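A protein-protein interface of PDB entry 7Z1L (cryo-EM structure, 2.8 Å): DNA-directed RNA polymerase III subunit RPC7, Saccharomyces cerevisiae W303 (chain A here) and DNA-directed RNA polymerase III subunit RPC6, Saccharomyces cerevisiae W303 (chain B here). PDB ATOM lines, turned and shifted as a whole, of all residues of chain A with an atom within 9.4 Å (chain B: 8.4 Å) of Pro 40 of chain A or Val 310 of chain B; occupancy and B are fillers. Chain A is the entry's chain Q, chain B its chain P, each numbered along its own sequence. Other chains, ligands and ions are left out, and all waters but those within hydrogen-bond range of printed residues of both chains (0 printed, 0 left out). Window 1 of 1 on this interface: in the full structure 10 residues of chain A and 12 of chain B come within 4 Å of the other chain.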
ATOM      1  N   PRO A  37       1.179 -17.039  28.533  1.00  0.00           N
ATOM      2  CA  PRO A  37       1.095 -15.592  28.314  1.00  0.00           C
ATOM      3  C   PRO A  37      -0.344 -15.100  28.298  1.00  0.00           C
ATOM      4  O   PRO A  37      -1.298 -15.866  28.148  1.00  0.00           O
ATOM      5  CB  PRO A  37       1.758 -15.407  26.947  1.00  0.00           C
ATOM      6  CG  PRO A  37       1.547 -16.710  26.260  1.00  0.00           C
ATOM      7  CD  PRO A  37       1.595 -17.765  27.322  1.00  0.00           C
ATOM      8  N   SER A  38      -0.488 -13.782  28.460  1.00  0.00           N
ATOM      9  CA  SER A  38      -1.808 -13.170  28.517  1.00  0.00           C
ATOM     10  C   SER A  38      -1.906 -11.872  27.721  1.00  0.00           C
ATOM     11  O   SER A  38      -2.900 -11.150  27.869  1.00  0.00           O
ATOM     12  CB  SER A  38      -2.208 -12.906  29.973  1.00  0.00           C
ATOM     13  OG  SER A  38      -2.235 -14.110  30.720  1.00  0.00           O
ATOM     14  N   ILE A  39      -0.921 -11.550  26.889  1.00  0.00           N
ATOM     15  CA  ILE A  39      -0.924 -10.300  26.132  1.00  0.00           C
ATOM     16  C   ILE A  39      -0.920 -10.622  24.642  1.00  0.00           C
ATOM     17  O   ILE A  39       0.153 -10.826  24.055  1.00  0.00           O
ATOM     18  CB  ILE A  39       0.275  -9.416  26.512  1.00  0.00           C
ATOM     19  CG1 ILE A  39       0.383  -9.284  28.031  1.00  0.00           C
ATOM     20  CG2 ILE A  39       0.151  -8.047  25.871  1.00  0.00           C
ATOM     21  CD1 ILE A  39       1.545  -8.440  28.492  1.00  0.00           C
ATOM     22  N   PRO A  40      -2.079 -10.680  23.995  1.00  0.00           N
ATOM     23  CA  PRO A  40      -2.119 -11.069  22.583  1.00  0.00           C
ATOM     24  C   PRO A  40      -1.938  -9.890  21.641  1.00  0.00           C
ATOM     25  O   PRO A  40      -2.341  -8.760  21.923  1.00  0.00           O
ATOM     26  CB  PRO A  40      -3.519 -11.673  22.434  1.00  0.00           C
ATOM     27  CG  PRO A  40      -4.340 -10.920  23.424  1.00  0.00           C
ATOM     28  CD  PRO A  40      -3.428 -10.545  24.569  1.00  0.00           C
ATOM     29  N   LEU A  41      -1.310 -10.179  20.503  1.00  0.00           N
ATOM     30  CA  LEU A  41      -1.209  -9.216  19.424  1.00  0.00           C
ATOM     31  C   LEU A  41      -2.560  -9.085  18.717  1.00  0.00           C
ATOM     32  O   LEU A  41      -3.370 -10.013  18.737  1.00  0.00           O
ATOM     33  CB  LEU A  41      -0.123  -9.648  18.439  1.00  0.00           C
ATOM     34  CG  LEU A  41       1.306  -9.225  18.783  1.00  0.00           C
ATOM     35  CD1 LEU A  41       2.312 -10.100  18.059  1.00  0.00           C
ATOM     36  CD2 LEU A  41       1.530  -7.765  18.443  1.00  0.00           C
ATOM     37  N   PRO A  42      -2.829  -7.939  18.079  1.00  0.00           N
ATOM     38  CA  PRO A  42      -4.132  -7.749  17.420  1.00  0.00           C
ATOM     39  C   PRO A  42      -4.290  -8.492  16.104  1.00  0.00           C
ATOM     40  O   PRO A  42      -5.242  -8.209  15.369  1.00  0.00           O
ATOM     41  CB  PRO A  42      -4.194  -6.230  17.186  1.00  0.00           C
ATOM     42  CG  PRO A  42      -3.065  -5.651  17.950  1.00  0.00           C
ATOM     43  CD  PRO A  42      -2.029  -6.705  18.058  1.00  0.00           C
ATOM     44  N   ILE A  43      -3.401  -9.425  15.779  1.00  0.00           N
ATOM     45  CA  ILE A  43      -3.422 -10.114  14.496  1.00  0.00           C
ATOM     46  C   ILE A  43      -4.391 -11.287  14.537  1.00  0.00           C
ATOM     47  O   ILE A  43      -4.605 -11.964  13.526  1.00  0.00           O
ATOM     48  CB  ILE A  43      -2.015 -10.609  14.131  1.00  0.00           C
ATOM     49  CG1 ILE A  43      -1.559 -11.610  15.183  1.00  0.00           C
ATOM     50  CG2 ILE A  43      -1.045  -9.447  14.062  1.00  0.00           C
ATOM     51  CD1 ILE A  43      -0.249 -12.223  14.893  1.00  0.00           C
ATOM     52  N   ASN A  44      -4.982 -11.542  15.703  1.00  0.00           N
ATOM     53  CA  ASN A  44      -5.766 -12.751  15.923  1.00  0.00           C
ATOM     54  C   ASN A  44      -7.240 -12.575  15.581  1.00  0.00           C
ATOM     55  O   ASN A  44      -8.090 -13.290  16.128  1.00  0.00           O
ATOM     56  CB  ASN A  44      -5.602 -13.214  17.370  1.00  0.00           C
ATOM     57  CG  ASN A  44      -4.175 -13.089  17.860  1.00  0.00           C
ATOM     58  OD1 ASN A  44      -3.916 -12.490  18.903  1.00  0.00           O
ATOM     59  ND2 ASN A  44      -3.240 -13.655  17.111  1.00  0.00           N
ATOM     60  N   GLY A  45      -7.570 -11.647  14.685  1.00  0.00           N
ATOM     61  CA  GLY A  45      -8.941 -11.436  14.289  1.00  0.00           C
ATOM     62  C   GLY A  45      -9.404 -12.445  13.261  1.00  0.00           C
ATOM     63  O   GLY A  45      -8.676 -13.363  12.858  1.00  0.00           O
ATOM     64  N   PHE B 300     -10.843  -7.634  16.233  1.00  0.00           N
ATOM     65  CA  PHE B 300     -11.549  -8.325  17.300  1.00  0.00           C
ATOM     66  C   PHE B 300     -10.634  -9.330  17.991  1.00  0.00           C
ATOM     67  O   PHE B 300      -9.747  -9.911  17.359  1.00  0.00           O
ATOM     68  CB  PHE B 300     -12.771  -9.052  16.743  1.00  0.00           C
ATOM     69  CG  PHE B 300     -13.788  -8.139  16.120  1.00  0.00           C
ATOM     70  CD1 PHE B 300     -14.464  -7.208  16.889  1.00  0.00           C
ATOM     71  CD2 PHE B 300     -14.068  -8.217  14.767  1.00  0.00           C
ATOM     72  CE1 PHE B 300     -15.401  -6.367  16.318  1.00  0.00           C
ATOM     73  CE2 PHE B 300     -15.003  -7.380  14.190  1.00  0.00           C
ATOM     74  CZ  PHE B 300     -15.671  -6.454  14.967  1.00  0.00           C
ATOM     75  N   PRO B 301     -10.823  -9.539  19.296  1.00  0.00           N
ATOM     76  CA  PRO B 301     -10.050 -10.574  19.992  1.00  0.00           C
ATOM     77  C   PRO B 301     -10.411 -11.964  19.491  1.00  0.00           C
ATOM     78  O   PRO B 301     -11.530 -12.216  19.040  1.00  0.00           O
ATOM     79  CB  PRO B 301     -10.447 -10.388  21.462  1.00  0.00           C
ATOM     80  CG  PRO B 301     -11.009  -9.005  21.542  1.00  0.00           C
ATOM     81  CD  PRO B 301     -11.660  -8.760  20.221  1.00  0.00           C
ATOM     82  N   ALA B 302      -9.440 -12.869  19.571  1.00  0.00           N
ATOM     83  CA  ALA B 302      -9.641 -14.228  19.091  1.00  0.00           C
ATOM     84  C   ALA B 302     -10.593 -14.994  20.000  1.00  0.00           C
ATOM     85  O   ALA B 302     -10.733 -14.695  21.189  1.00  0.00           O
ATOM     86  CB  ALA B 302      -8.310 -14.970  19.005  1.00  0.00           C
ATOM     87  N   ASP B 306      -8.513 -21.576  21.212  1.00  0.00           N
ATOM     88  CA  ASP B 306      -7.800 -21.528  19.942  1.00  0.00           C
ATOM     89  C   ASP B 306      -6.317 -21.726  20.219  1.00  0.00           C
ATOM     90  O   ASP B 306      -5.709 -20.939  20.952  1.00  0.00           O
ATOM     91  CB  ASP B 306      -8.047 -20.201  19.223  1.00  0.00           C
ATOM     92  CG  ASP B 306      -7.592 -20.227  17.779  1.00  0.00           C
ATOM     93  OD1 ASP B 306      -7.548 -19.150  17.149  1.00  0.00           O
ATOM     94  OD2 ASP B 306      -7.279 -21.324  17.272  1.00  0.00           O
ATOM     95  N   LYS B 307      -5.740 -22.777  19.635  1.00  0.00           N
ATOM     96  CA  LYS B 307      -4.355 -23.123  19.938  1.00  0.00           C
ATOM     97  C   LYS B 307      -3.378 -22.167  19.268  1.00  0.00           C
ATOM     98  O   LYS B 307      -2.391 -21.747  19.884  1.00  0.00           O
ATOM     99  CB  LYS B 307      -4.068 -24.562  19.513  1.00  0.00           C
ATOM    100  CG  LYS B 307      -4.545 -25.617  20.497  1.00  0.00           C
ATOM    101  CD  LYS B 307      -5.955 -26.080  20.173  1.00  0.00           C
ATOM    102  CE  LYS B 307      -6.319 -27.332  20.952  1.00  0.00           C
ATOM    103  NZ  LYS B 307      -7.690 -27.807  20.615  1.00  0.00           N
ATOM    104  N   GLU B 308      -3.631 -21.809  18.010  1.00  0.00           N
ATOM    105  CA  GLU B 308      -2.668 -21.046  17.216  1.00  0.00           C
ATOM    106  C   GLU B 308      -2.997 -19.555  17.285  1.00  0.00           C
ATOM    107  O   GLU B 308      -3.346 -18.905  16.299  1.00  0.00           O
ATOM    108  CB  GLU B 308      -2.645 -21.552  15.782  1.00  0.00           C
ATOM    109  CG  GLU B 308      -2.367 -23.039  15.657  1.00  0.00           C
ATOM    110  CD  GLU B 308      -3.635 -23.862  15.626  1.00  0.00           C
ATOM    111  OE1 GLU B 308      -4.728 -23.261  15.681  1.00  0.00           O
ATOM    112  OE2 GLU B 308      -3.542 -25.104  15.549  1.00  0.00           O
ATOM    113  N   VAL B 309      -2.871 -19.019  18.494  1.00  0.00           N
ATOM    114  CA  VAL B 309      -3.059 -17.600  18.762  1.00  0.00           C
ATOM    115  C   VAL B 309      -1.726 -17.027  19.233  1.00  0.00           C
ATOM    116  O   VAL B 309      -0.992 -17.679  19.986  1.00  0.00           O
ATOM    117  CB  VAL B 309      -4.202 -17.363  19.771  1.00  0.00           C
ATOM    118  CG1 VAL B 309      -3.885 -17.944  21.131  1.00  0.00           C
ATOM    119  CG2 VAL B 309      -4.517 -15.885  19.892  1.00  0.00           C
ATOM    120  N   VAL B 310      -1.386 -15.841  18.737  1.00  0.00           N
ATOM    121  CA  VAL B 310      -0.055 -15.271  18.907  1.00  0.00           C
ATOM    122  C   VAL B 310      -0.072 -14.285  20.065  1.00  0.00           C
ATOM    123  O   VAL B 310      -0.918 -13.384  20.114  1.00  0.00           O
ATOM    124  CB  VAL B 310       0.416 -14.592  17.611  1.00  0.00           C
ATOM    125  CG1 VAL B 310       1.698 -13.811  17.845  1.00  0.00           C
ATOM    126  CG2 VAL B 310       0.604 -15.619  16.510  1.00  0.00           C
ATOM    127  N   TYR B 311       0.863 -14.449  20.998  1.00  0.00           N
ATOM    128  CA  TYR B 311       0.980 -13.585  22.165  1.00  0.00           C
ATOM    129  C   TYR B 311       2.264 -12.777  22.083  1.00  0.00           C
ATOM    130  O   TYR B 311       3.322 -13.315  21.739  1.00  0.00           O
ATOM    131  CB  TYR B 311       0.973 -14.392  23.462  1.00  0.00           C
ATOM    132  CG  TYR B 311      -0.333 -15.074  23.776  1.00  0.00           C
ATOM    133  CD1 TYR B 311      -1.333 -14.412  24.474  1.00  0.00           C
ATOM    134  CD2 TYR B 311      -0.553 -16.388  23.403  1.00  0.00           C
ATOM    135  CE1 TYR B 311      -2.524 -15.037  24.771  1.00  0.00           C
ATOM    136  CE2 TYR B 311      -1.735 -17.022  23.700  1.00  0.00           C
ATOM    137  CZ  TYR B 311      -2.721 -16.342  24.381  1.00  0.00           C
ATOM    138  OH  TYR B 311      -3.906 -16.973  24.675  1.00  0.00           O
ATOM    139  N   PHE B 312       2.168 -11.487  22.406  1.00  0.00           N
ATOM    140  CA  PHE B 312       3.360 -10.656  22.524  1.00  0.00           C
ATOM    141  C   PHE B 312       4.189 -11.037  23.744  1.00  0.00           C
ATOM    142  O   PHE B 312       5.422 -10.978  23.699  1.00  0.00           O
ATOM    143  CB  PHE B 312       2.959  -9.184  22.589  1.00  0.00           C
ATOM    144  CG  PHE B 312       4.115  -8.242  22.741  1.00  0.00           C
ATOM    145  CD1 PHE B 312       5.014  -8.054  21.706  1.00  0.00           C
ATOM    146  CD2 PHE B 312       4.294  -7.532  23.915  1.00  0.00           C
ATOM    147  CE1 PHE B 312       6.076  -7.183  21.843  1.00  0.00           C
ATOM    148  CE2 PHE B 312       5.352  -6.659  24.059  1.00  0.00           C
ATOM    149  CZ  PHE B 312       6.244  -6.484  23.021  1.00  0.00           C
ATOM    150  N   ASP B 313       3.530 -11.434  24.835  1.00  0.00           N
ATOM    151  CA  ASP B 313       4.219 -11.767  26.075  1.00  0.00           C
ATOM    152  C   ASP B 313       4.977 -13.085  26.001  1.00  0.00           C
ATOM    153  O   ASP B 313       5.811 -13.352  26.872  1.00  0.00           O
ATOM    154  CB  ASP B 313       3.215 -11.820  27.229  1.00  0.00           C
ATOM    155  CG  ASP B 313       3.864 -11.587  28.578  1.00  0.00           C
ATOM    156  OD1 ASP B 313       4.512 -10.536  28.755  1.00  0.00           O
ATOM    157  OD2 ASP B 313       3.724 -12.457  29.462  1.00  0.00           O
ATOM    158  N   GLU B 314       4.707 -13.908  24.995  1.00  0.00           N
ATOM    159  CA  GLU B 314       5.397 -15.180  24.858  1.00  0.00           C
ATOM    160  C   GLU B 314       6.826 -14.937  24.372  1.00  0.00           C
ATOM    161  O   GLU B 314       7.167 -13.846  23.902  1.00  0.00           O
ATOM    162  CB  GLU B 314       4.615 -16.087  23.904  1.00  0.00           C
ATOM    163  CG  GLU B 314       4.944 -17.565  23.977  1.00  0.00           C
ATOM    164  CD  GLU B 314       4.000 -18.402  23.139  1.00  0.00           C
ATOM    165  OE1 GLU B 314       3.111 -17.821  22.484  1.00  0.00           O
ATOM    166  OE2 GLU B 314       4.136 -19.641  23.144  1.00  0.00           O
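Tyr 311 of chain B touches Pro 37 of chain A (CG to CG, 3.5 Å). CB of Pro 37 of chain A touches CB of Asp 313 of chain B, 3.9 Å away. O of Ile 39 of chain A touches CA of Tyr 311 of chain B, at 3.4 Å. Asp 313 of chain B touches Ile 39 of chain A. O of Val 310 of chain B touches CA of Pro 40 of chain A (3.6 Å). Pro 40 of chain A touches Tyr 311 of chain B (N to CD1, 3.8 Å). Ile 43 of chain A touches Val 310 of chain B. Asn 44 of chain A touches Phe 300 of chain B. Val 309 of chain B touches Asn 44 of chain A. Gly 45 of chain A touches Phe 300 of chain B (CA to O, 3.5 Å).
The backbone carbonyl oxygen (O) of Leu 41 of chain A sits close to the side-chain amide oxygen (OD1) of Asn 44 of chain A (2.5 Å).
Of the 12 printed residues of chain B, 8 touch a printed residue of chain A. Printed residues of chain B that touch a printed residue of chain A: Phe 300, Ala 302, Val 309, Val 310, Tyr 311, Phe 312, Asp 313 and Glu 314. Of the 9 printed residues of chain A, 7 touch a printed residue of chain B. Printed residues of chain A that touch a printed residue of chain B: Pro 37, Ile 39, Pro 40, Leu 41, Ile 43, Asn 44 and Gly 45. Hydrophobic or aromatic side chains of chain A within 4 Å of the printed part of chain B: Pro 37, Ile 39, Pro 40, Leu 41 and Ile 43. Among the printed residues, no Asp or Glu carboxylate lies within 4 Å of a Lys or Arg side-chain nitrogen of the other chain.
The backbone carbonyl oxygen (O) of Ile 39 of chain A lies within hydrogen-bond range of the backbone NH (N) of Phe 312 of chain B, at 2.7 Å. O of Val 310 of chain B is in hydrogen-bond range of N of Leu 41 of chain A (3.3 Å). The backbone NH of Val 310 of chain B lies close to the side-chain amide nitrogen of Asn 44 of chain A.
Pro 40 of chain A touches two residues of chain B. Val 310 of chain B touches just these residues of chain A: Pro 40 (3.6 Å), Leu 41 (3.3 Å), Ile 43 (3.7 Å) and Asn 44 (3.3 Å). Val 309 of chain B touches just one residue of chain A: Asn 44. Of the printed residues of chain A, Glu 314 of chain B touches Pro 37. Printed residues of chain B within 4 Å of Leu 41 of chain A: Val 310 (3.3 Å). Of the printed residues of chain A, Phe 300 of chain B touches Asn 44 (3.96 Å) and Gly 45 (3.5 Å). Pro 301 of chain B touches none of the printed residues of chain A. Ser 38 of chain A touches none of the printed residues of chain B. The nearest residue of chain A that does not touch Val 310 of chain B is Ile 39 of chain A (4.8 Å).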
